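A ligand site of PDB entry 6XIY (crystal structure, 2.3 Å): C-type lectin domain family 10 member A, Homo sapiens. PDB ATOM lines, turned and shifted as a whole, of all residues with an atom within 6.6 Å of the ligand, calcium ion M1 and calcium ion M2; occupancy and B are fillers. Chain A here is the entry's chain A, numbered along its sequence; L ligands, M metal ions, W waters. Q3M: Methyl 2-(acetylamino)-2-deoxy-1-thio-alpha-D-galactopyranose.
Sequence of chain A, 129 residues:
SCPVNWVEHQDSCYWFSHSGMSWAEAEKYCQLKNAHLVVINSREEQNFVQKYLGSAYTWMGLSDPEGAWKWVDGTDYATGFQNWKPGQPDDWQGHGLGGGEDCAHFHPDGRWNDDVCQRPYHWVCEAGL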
ATOM      1  N   TYR A  57      16.263  10.694 -10.182  1.00  0.00           N
ATOM      2  CA  TYR A  57      15.076  11.322 -10.827  1.00  0.00           C
ATOM      3  C   TYR A  57      13.835  10.571 -10.361  1.00  0.00           C
ATOM      4  O   TYR A  57      13.878   9.329 -10.370  1.00  0.00           O
ATOM      5  CB  TYR A  57      15.207  11.330 -12.355  1.00  0.00           C
ATOM      6  CG  TYR A  57      16.387  12.118 -12.869  1.00  0.00           C
ATOM      7  CD1 TYR A  57      16.864  13.237 -12.197  1.00  0.00           C
ATOM      8  CD2 TYR A  57      17.047  11.728 -14.019  1.00  0.00           C
ATOM      9  CE1 TYR A  57      17.956  13.937 -12.658  1.00  0.00           C
ATOM     10  CE2 TYR A  57      18.119  12.440 -14.526  1.00  0.00           C
ATOM     11  CZ  TYR A  57      18.579  13.554 -13.842  1.00  0.00           C
ATOM     12  OH  TYR A  57      19.609  14.251 -14.360  1.00  0.00           O
ATOM     13  N   ASP A  64       1.255  16.929 -18.884  1.00  0.00           N
ATOM     14  CA  ASP A  64       0.625  17.843 -19.882  1.00  0.00           C
ATOM     15  C   ASP A  64       0.431  17.116 -21.210  1.00  0.00           C
ATOM     16  O   ASP A  64       0.668  17.718 -22.251  1.00  0.00           O
ATOM     17  CB  ASP A  64       1.457  19.122 -20.085  1.00  0.00           C
ATOM     18  CG  ASP A  64       2.739  18.990 -20.892  1.00  0.00           C
ATOM     19  OD1 ASP A  64       3.301  17.873 -20.988  1.00  0.00           O
ATOM     20  OD2 ASP A  64       3.221  19.993 -21.456  1.00  0.00           O
ATOM     21  N   PRO A  65      -0.028  15.846 -21.246  1.00  0.00           N
ATOM     22  CA  PRO A  65      -0.151  15.121 -22.519  1.00  0.00           C
ATOM     23  C   PRO A  65      -1.167  15.811 -23.449  1.00  0.00           C
ATOM     24  O   PRO A  65      -0.929  15.866 -24.647  1.00  0.00           O
ATOM     25  CB  PRO A  65      -0.597  13.697 -22.124  1.00  0.00           C
ATOM     26  CG  PRO A  65      -1.221  13.880 -20.755  1.00  0.00           C
ATOM     27  CD  PRO A  65      -0.453  15.018 -20.109  1.00  0.00           C
ATOM     28  N   GLY A  67      -1.764  19.090 -23.617  1.00  0.00           N
ATOM     29  CA  GLY A  67      -1.373  20.490 -23.933  1.00  0.00           C
ATOM     30  C   GLY A  67      -1.164  21.379 -22.710  1.00  0.00           C
ATOM     31  O   GLY A  67      -0.228  22.205 -22.772  1.00  0.00           O
ATOM     32  N   TRP A  69      -0.599  21.728 -18.336  1.00  0.00           N
ATOM     33  CA  TRP A  69      -0.108  21.025 -17.115  1.00  0.00           C
ATOM     34  C   TRP A  69      -1.254  20.747 -16.141  1.00  0.00           C
ATOM     35  O   TRP A  69      -2.015  21.665 -15.889  1.00  0.00           O
ATOM     36  CB  TRP A  69       1.013  21.797 -16.437  1.00  0.00           C
ATOM     37  CG  TRP A  69       2.280  21.695 -17.214  1.00  0.00           C
ATOM     38  CD1 TRP A  69       2.790  22.604 -18.091  1.00  0.00           C
ATOM     39  CD2 TRP A  69       3.161  20.560 -17.235  1.00  0.00           C
ATOM     40  NE1 TRP A  69       3.951  22.124 -18.625  1.00  0.00           N
ATOM     41  CE2 TRP A  69       4.196  20.866 -18.139  1.00  0.00           C
ATOM     42  CE3 TRP A  69       3.157  19.311 -16.604  1.00  0.00           C
ATOM     43  CZ2 TRP A  69       5.227  19.976 -18.409  1.00  0.00           C
ATOM     44  CZ3 TRP A  69       4.187  18.444 -16.874  1.00  0.00           C
ATOM     45  CH2 TRP A  69       5.204  18.767 -17.766  1.00  0.00           C
ATOM     46  N   LYS A  85      13.219  23.740 -12.661  1.00  0.00           N
ATOM     47  CA  LYS A  85      14.626  24.005 -13.036  1.00  0.00           C
ATOM     48  C   LYS A  85      14.668  25.217 -13.965  1.00  0.00           C
ATOM     49  O   LYS A  85      13.730  25.392 -14.734  1.00  0.00           O
ATOM     50  CB  LYS A  85      15.212  22.809 -13.799  1.00  0.00           C
ATOM     51  CG  LYS A  85      15.900  21.748 -12.963  1.00  0.00           C
ATOM     52  CD  LYS A  85      17.237  22.164 -12.401  1.00  0.00           C
ATOM     53  CE  LYS A  85      18.053  20.962 -11.955  1.00  0.00           C
ATOM     54  NZ  LYS A  85      18.871  21.229 -10.752  1.00  0.00           N
ATOM     55  N   GLY A  87      14.990  27.002 -17.282  1.00  0.00           N
ATOM     56  CA  GLY A  87      14.784  26.574 -18.675  1.00  0.00           C
ATOM     57  C   GLY A  87      13.645  25.568 -18.820  1.00  0.00           C
ATOM     58  O   GLY A  87      13.268  25.278 -19.953  1.00  0.00           O
ATOM     59  N   GLN A  88      13.090  25.053 -17.718  1.00  0.00           N
ATOM     60  CA  GLN A  88      11.991  24.059 -17.752  1.00  0.00           C
ATOM     61  C   GLN A  88      10.683  24.742 -17.370  1.00  0.00           C
ATOM     62  O   GLN A  88      10.682  25.758 -16.666  1.00  0.00           O
ATOM     63  CB  GLN A  88      12.392  22.840 -16.904  1.00  0.00           C
ATOM     64  CG  GLN A  88      13.801  22.331 -17.196  1.00  0.00           C
ATOM     65  CD  GLN A  88      13.955  21.670 -18.561  1.00  0.00           C
ATOM     66  OE1 GLN A  88      12.977  21.374 -19.248  1.00  0.00           O
ATOM     67  NE2 GLN A  88      15.198  21.369 -18.944  1.00  0.00           N
ATOM     68  N   PRO A  89       9.518  24.239 -17.840  1.00  0.00           N
ATOM     69  CA  PRO A  89       9.467  23.090 -18.747  1.00  0.00           C
ATOM     70  C   PRO A  89       9.758  23.530 -20.196  1.00  0.00           C
ATOM     71  O   PRO A  89       9.579  24.685 -20.452  1.00  0.00           O
ATOM     72  CB  PRO A  89       8.032  22.599 -18.568  1.00  0.00           C
ATOM     73  CG  PRO A  89       7.219  23.833 -18.206  1.00  0.00           C
ATOM     74  CD  PRO A  89       8.193  24.778 -17.526  1.00  0.00           C
ATOM     75  N   ASP A  90      10.266  22.639 -21.053  1.00  0.00           N
ATOM     76  CA  ASP A  90      10.736  23.001 -22.429  1.00  0.00           C
ATOM     77  C   ASP A  90      10.106  22.098 -23.507  1.00  0.00           C
ATOM     78  O   ASP A  90      10.404  22.348 -24.678  1.00  0.00           O
ATOM     79  CB  ASP A  90      12.260  22.932 -22.562  1.00  0.00           C
ATOM     80  CG  ASP A  90      12.875  21.561 -22.250  1.00  0.00           C
ATOM     81  OD1 ASP A  90      12.138  20.610 -21.791  1.00  0.00           O
ATOM     82  OD2 ASP A  90      14.102  21.453 -22.456  1.00  0.00           O
ATOM     83  N   ASP A  91       9.368  21.053 -23.129  1.00  0.00           N
ATOM     84  CA  ASP A  91       8.778  20.053 -24.059  1.00  0.00           C
ATOM     85  C   ASP A  91       9.824  19.598 -25.114  1.00  0.00           C
ATOM     86  O   ASP A  91       9.461  19.469 -26.306  1.00  0.00           O
ATOM     87  CB  ASP A  91       7.522  20.651 -24.704  1.00  0.00           C
ATOM     88  CG  ASP A  91       6.583  19.610 -25.325  1.00  0.00           C
ATOM     89  OD1 ASP A  91       6.238  18.599 -24.622  1.00  0.00           O
ATOM     90  OD2 ASP A  91       6.173  19.842 -26.476  1.00  0.00           O
ATOM     91  N   TRP A  92      11.084  19.365 -24.720  1.00  0.00           N
ATOM     92  CA  TRP A  92      12.232  19.035 -25.632  1.00  0.00           C
ATOM     93  C   TRP A  92      11.887  17.857 -26.540  1.00  0.00           C
ATOM     94  O   TRP A  92      11.264  16.902 -26.015  1.00  0.00           O
ATOM     95  CB  TRP A  92      13.445  18.688 -24.787  1.00  0.00           C
ATOM     96  CG  TRP A  92      14.753  18.597 -25.499  1.00  0.00           C
ATOM     97  CD1 TRP A  92      15.275  19.502 -26.369  1.00  0.00           C
ATOM     98  CD2 TRP A  92      15.759  17.589 -25.312  1.00  0.00           C
ATOM     99  NE1 TRP A  92      16.519  19.098 -26.769  1.00  0.00           N
ATOM    100  CE2 TRP A  92      16.849  17.929 -26.132  1.00  0.00           C
ATOM    101  CE3 TRP A  92      15.848  16.416 -24.549  1.00  0.00           C
ATOM    102  CZ2 TRP A  92      18.011  17.152 -26.213  1.00  0.00           C
ATOM    103  CZ3 TRP A  92      17.003  15.653 -24.611  1.00  0.00           C
ATOM    104  CH2 TRP A  92      18.071  16.018 -25.436  1.00  0.00           C
ATOM    105  N   GLY A 100       7.392  15.321 -27.441  1.00  0.00           N
ATOM    106  CA  GLY A 100       8.169  16.215 -26.566  1.00  0.00           C
ATOM    107  C   GLY A 100       8.426  15.553 -25.222  1.00  0.00           C
ATOM    108  O   GLY A 100       8.981  14.419 -25.188  1.00  0.00           O
ATOM    109  N   GLU A 101       8.037  16.221 -24.147  1.00  0.00           N
ATOM    110  CA  GLU A 101       8.204  15.780 -22.744  1.00  0.00           C
ATOM    111  C   GLU A 101       6.925  16.158 -21.987  1.00  0.00           C
ATOM    112  O   GLU A 101       6.562  17.335 -22.014  1.00  0.00           O
ATOM    113  CB  GLU A 101       9.467  16.431 -22.153  1.00  0.00           C
ATOM    114  CG  GLU A 101      10.766  15.987 -22.823  1.00  0.00           C
ATOM    115  CD  GLU A 101      11.998  16.606 -22.185  1.00  0.00           C
ATOM    116  OE1 GLU A 101      11.871  17.781 -21.751  1.00  0.00           O
ATOM    117  OE2 GLU A 101      13.078  15.913 -22.084  1.00  0.00           O
ATOM    118  N   ASP A 102       6.230  15.183 -21.412  1.00  0.00           N
ATOM    119  CA  ASP A 102       4.847  15.363 -20.924  1.00  0.00           C
ATOM    120  C   ASP A 102       4.688  14.937 -19.472  1.00  0.00           C
ATOM    121  O   ASP A 102       3.561  14.969 -19.005  1.00  0.00           O
ATOM    122  CB  ASP A 102       3.870  14.586 -21.815  1.00  0.00           C
ATOM    123  CG  ASP A 102       3.830  15.184 -23.211  1.00  0.00           C
ATOM    124  OD1 ASP A 102       4.355  16.366 -23.389  1.00  0.00           O
ATOM    125  OD2 ASP A 102       3.315  14.492 -24.117  1.00  0.00           O
ATOM    126  N   CYS A 103       5.782  14.619 -18.770  1.00  0.00           N
ATOM    127  CA  CYS A 103       5.768  14.104 -17.379  1.00  0.00           C
ATOM    128  C   CYS A 103       6.873  14.809 -16.583  1.00  0.00           C
ATOM    129  O   CYS A 103       7.966  14.976 -17.137  1.00  0.00           O
ATOM    130  CB  CYS A 103       5.964  12.595 -17.380  1.00  0.00           C
ATOM    131  SG  CYS A 103       4.536  11.696 -18.038  1.00  0.00           S
ATOM    132  N   HIS A 105       9.336  15.398 -13.136  1.00  0.00           N
ATOM    133  CA  HIS A 105      10.059  14.648 -12.097  1.00  0.00           C
ATOM    134  C   HIS A 105      10.881  15.620 -11.295  1.00  0.00           C
ATOM    135  O   HIS A 105      11.236  16.668 -11.823  1.00  0.00           O
ATOM    136  CB  HIS A 105      10.928  13.558 -12.739  1.00  0.00           C
ATOM    137  CG  HIS A 105      12.067  14.074 -13.538  1.00  0.00           C
ATOM    138  ND1 HIS A 105      13.327  14.259 -12.995  1.00  0.00           N
ATOM    139  CD2 HIS A 105      12.164  14.409 -14.842  1.00  0.00           C
ATOM    140  CE1 HIS A 105      14.148  14.704 -13.935  1.00  0.00           C
ATOM    141  NE2 HIS A 105      13.460  14.791 -15.080  1.00  0.00           N
ATOM    142  N   HIS A 107      14.572  16.541  -9.819  1.00  0.00           N
ATOM    143  CA  HIS A 107      16.034  16.323  -9.707  1.00  0.00           C
ATOM    144  C   HIS A 107      16.340  16.094  -8.228  1.00  0.00           C
ATOM    145  O   HIS A 107      15.521  16.405  -7.357  1.00  0.00           O
ATOM    146  CB  HIS A 107      16.823  17.504 -10.279  1.00  0.00           C
ATOM    147  CG  HIS A 107      16.866  17.576 -11.769  1.00  0.00           C
ATOM    148  ND1 HIS A 107      18.042  17.535 -12.476  1.00  0.00           N
ATOM    149  CD2 HIS A 107      15.881  17.757 -12.684  1.00  0.00           C
ATOM    150  CE1 HIS A 107      17.803  17.669 -13.766  1.00  0.00           C
ATOM    151  NE2 HIS A 107      16.469  17.802 -13.923  1.00  0.00           N
ATOM    152  N   ASN A 113      11.779  18.998 -13.693  1.00  0.00           N
ATOM    153  CA  ASN A 113      12.035  18.958 -15.156  1.00  0.00           C
ATOM    154  C   ASN A 113      10.875  18.203 -15.818  1.00  0.00           C
ATOM    155  O   ASN A 113      10.303  17.327 -15.163  1.00  0.00           O
ATOM    156  CB  ASN A 113      13.393  18.331 -15.474  1.00  0.00           C
ATOM    157  CG  ASN A 113      13.553  18.036 -16.954  1.00  0.00           C
ATOM    158  OD1 ASN A 113      13.379  18.928 -17.793  1.00  0.00           O
ATOM    159  ND2 ASN A 113      13.823  16.782 -17.286  1.00  0.00           N
ATOM    160  N   ASP A 114      10.527  18.540 -17.055  1.00  0.00           N
ATOM    161  CA  ASP A 114       9.642  17.692 -17.898  1.00  0.00           C
ATOM    162  C   ASP A 114      10.512  16.738 -18.733  1.00  0.00           C
ATOM    163  O   ASP A 114      11.610  17.170 -19.214  1.00  0.00           O
ATOM    164  CB  ASP A 114       8.709  18.524 -18.786  1.00  0.00           C
ATOM    165  CG  ASP A 114       9.385  19.478 -19.752  1.00  0.00           C
ATOM    166  OD1 ASP A 114      10.596  19.842 -19.507  1.00  0.00           O
ATOM    167  OD2 ASP A 114       8.704  19.889 -20.739  1.00  0.00           O
ATOM    168  N   ASP A 115      10.080  15.487 -18.788  1.00  0.00           N
ATOM    169  CA  ASP A 115      10.835  14.361 -19.391  1.00  0.00           C
ATOM    170  C   ASP A 115       9.826  13.415 -20.042  1.00  0.00           C
ATOM    171  O   ASP A 115       8.571  13.637 -19.909  1.00  0.00           O
ATOM    172  CB  ASP A 115      11.726  13.635 -18.374  1.00  0.00           C
ATOM    173  CG  ASP A 115      13.079  13.141 -18.921  1.00  0.00           C
ATOM    174  OD1 ASP A 115      13.140  12.782 -20.118  1.00  0.00           O
ATOM    175  OD2 ASP A 115      14.065  13.124 -18.140  1.00  0.00           O
ATOM    176  N   VAL A 116      10.391  12.420 -20.713  1.00  0.00           N
ATOM    177  CA  VAL A 116       9.686  11.382 -21.503  1.00  0.00           C
ATOM    178  C   VAL A 116       9.079  10.417 -20.499  1.00  0.00           C
ATOM    179  O   VAL A 116       9.838   9.878 -19.670  1.00  0.00           O
ATOM    180  CB  VAL A 116      10.675  10.696 -22.468  1.00  0.00           C
ATOM    181  CG1 VAL A 116      10.014   9.565 -23.256  1.00  0.00           C
ATOM    182  CG2 VAL A 116      11.301  11.720 -23.412  1.00  0.00           C
ATOM    183  N   TYR A 121      11.798   5.787 -13.752  1.00  0.00           N
ATOM    184  CA  TYR A 121      12.278   6.672 -12.664  1.00  0.00           C
ATOM    185  C   TYR A 121      11.649   6.232 -11.340  1.00  0.00           C
ATOM    186  O   TYR A 121      10.628   5.504 -11.338  1.00  0.00           O
ATOM    187  CB  TYR A 121      11.898   8.132 -12.956  1.00  0.00           C
ATOM    188  CG  TYR A 121      12.689   8.876 -14.004  1.00  0.00           C
ATOM    189  CD1 TYR A 121      13.900   8.421 -14.480  1.00  0.00           C
ATOM    190  CD2 TYR A 121      12.231  10.090 -14.492  1.00  0.00           C
ATOM    191  CE1 TYR A 121      14.630   9.136 -15.416  1.00  0.00           C
ATOM    192  CE2 TYR A 121      12.952  10.823 -15.418  1.00  0.00           C
ATOM    193  CZ  TYR A 121      14.167  10.350 -15.881  1.00  0.00           C
ATOM    194  OH  TYR A 121      14.891  11.056 -16.798  1.00  0.00           O
HETATM  195  C01 Q3M L   1      20.483  17.137 -21.491  1.00  0.00           C
HETATM  196  S02 Q3M L   1      18.895  16.590 -20.766  1.00  0.00           S
HETATM  197  C03 Q3M L   1      18.011  17.959 -19.870  1.00  0.00           C
HETATM  198  C04 Q3M L   1      17.932  19.249 -20.668  1.00  0.00           C
HETATM  199  C05 Q3M L   1      17.075  18.994 -21.915  1.00  0.00           C
HETATM  200  C06 Q3M L   1      17.111  20.260 -22.815  1.00  0.00           C
HETATM  201  O07 Q3M L   1      18.457  20.487 -23.197  1.00  0.00           O
HETATM  202  C08 Q3M L   1      15.633  18.548 -21.599  1.00  0.00           C
HETATM  203  O09 Q3M L   1      14.785  19.514 -20.977  1.00  0.00           O
HETATM  204  C10 Q3M L   1      15.574  17.349 -20.649  1.00  0.00           C
HETATM  205  O11 Q3M L   1      14.223  17.301 -20.201  1.00  0.00           O
HETATM  206  C12 Q3M L   1      16.549  17.549 -19.487  1.00  0.00           C
HETATM  207  N13 Q3M L   1      16.722  16.289 -18.784  1.00  0.00           N
HETATM  208  C14 Q3M L   1      16.851  16.286 -17.339  1.00  0.00           C
HETATM  209  C15 Q3M L   1      17.011  14.922 -16.673  1.00  0.00           C
HETATM  210  O16 Q3M L   1      16.766  17.298 -16.710  1.00  0.00           O
HETATM  211 CA    CA M   1      12.693  19.120 -20.031  1.00  0.00          CA
HETATM  212 CA    CA M   2       4.753  18.632 -22.759  1.00  0.00          CA
HETATM  213  O   HOH W   1      16.567  13.749 -19.699  1.00  0.00           O
HETATM  214  O   HOH W   2       6.270  20.136 -21.776  1.00  0.00           O
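A ring nitrogen (NE2) of His 107 lies within hydrogen-bond range of an oxygen (O16) of the ligand.
OD2 of Asp 115 lies within hydrogen-bond range of OH of Tyr 121, 2.6 Å away. O of Asp 115 is in hydrogen-bond range of N of Asp 102 (3.2 Å). The side-chain carboxylate (OD2) of Asp 114 sits at hydrogen-bond distance from the backbone NH (N) of Asp 91. The backbone NH (N) of Asp 115 is in hydrogen-bond range of the backbone carbonyl oxygen (O) of Cys 103 (2.7 Å). The side-chain carboxylate (OE1) of Glu 101 sits close to the backbone NH (N) of Trp 92, at 3.5 Å. The backbone NH of Trp 92 lies close to the side-chain carboxylate of Asp 90, at 3.4 Å. The backbone carbonyl oxygen (O) of Asn 113 is in hydrogen-bond range of the backbone NH (N) of His 105, at 3.0 Å.
Merely in contact with the ligand: Tyr 57, Trp 92, His 105 and Asp 115. Hydrophobic or aromatic side chains that line the ligand: Tyr 57, Trp 92, His 105 and His 107. Ten residues have an atom within 4 Å of the ligand: Tyr 57, Gln 88, Asp 90, Trp 92, Glu 101, His 105, His 107, Asn 113, Asp 114 and Asp 115. Along chain A the residues within 4 Å of the ligand span positions 57 to 115. The nearest printed residue that does not touch the ligand is Tyr 121 (4.4 Å).
Within 4 Å of calcium ion M2: Asp 64, Asp 91, Glu 101 and Asp 102.
Calcium ion M1 is bound by the side-chain carboxylate of Asp 114 (2.3 Å), an oxygen (O09) of the ligand (2.3 Å), the side-chain carboxylate of Glu 101 (2.3 Å), the side-chain amide oxygen of Asn 113 (2.3 Å), the side-chain carboxylate of Asp 90 (2.4 Å), the backbone carbonyl oxygen of Asp 114 (2.4 Å), an oxygen (O11) of the ligand (2.4 Å) and the side-chain amide oxygen of Gln 88 (2.4 Å). Calcium ion M1 has eight donor atoms within binding distance.
The backbone carbonyl oxygen (O) of Glu 101 binds calcium ion M2 (2.3 Å). Calcium ion M2 is bound by water W2 (2.4 Å). Calcium ion M2 is bound by OD1 of Asp 91. Calcium ion M2 is bound by OD1 of Asp 102, 2.4 Å away. Calcium ion M2 is bound by the side-chain carboxylate (OD1) of Asp 64, 2.4 Å away. OD2 of Asp 64 is bound to calcium ion M2, at 2.4 Å.
Water W1 bridges N13 of the ligand (2.7 Å) and OD2 of Asp 115 (3.0 Å).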
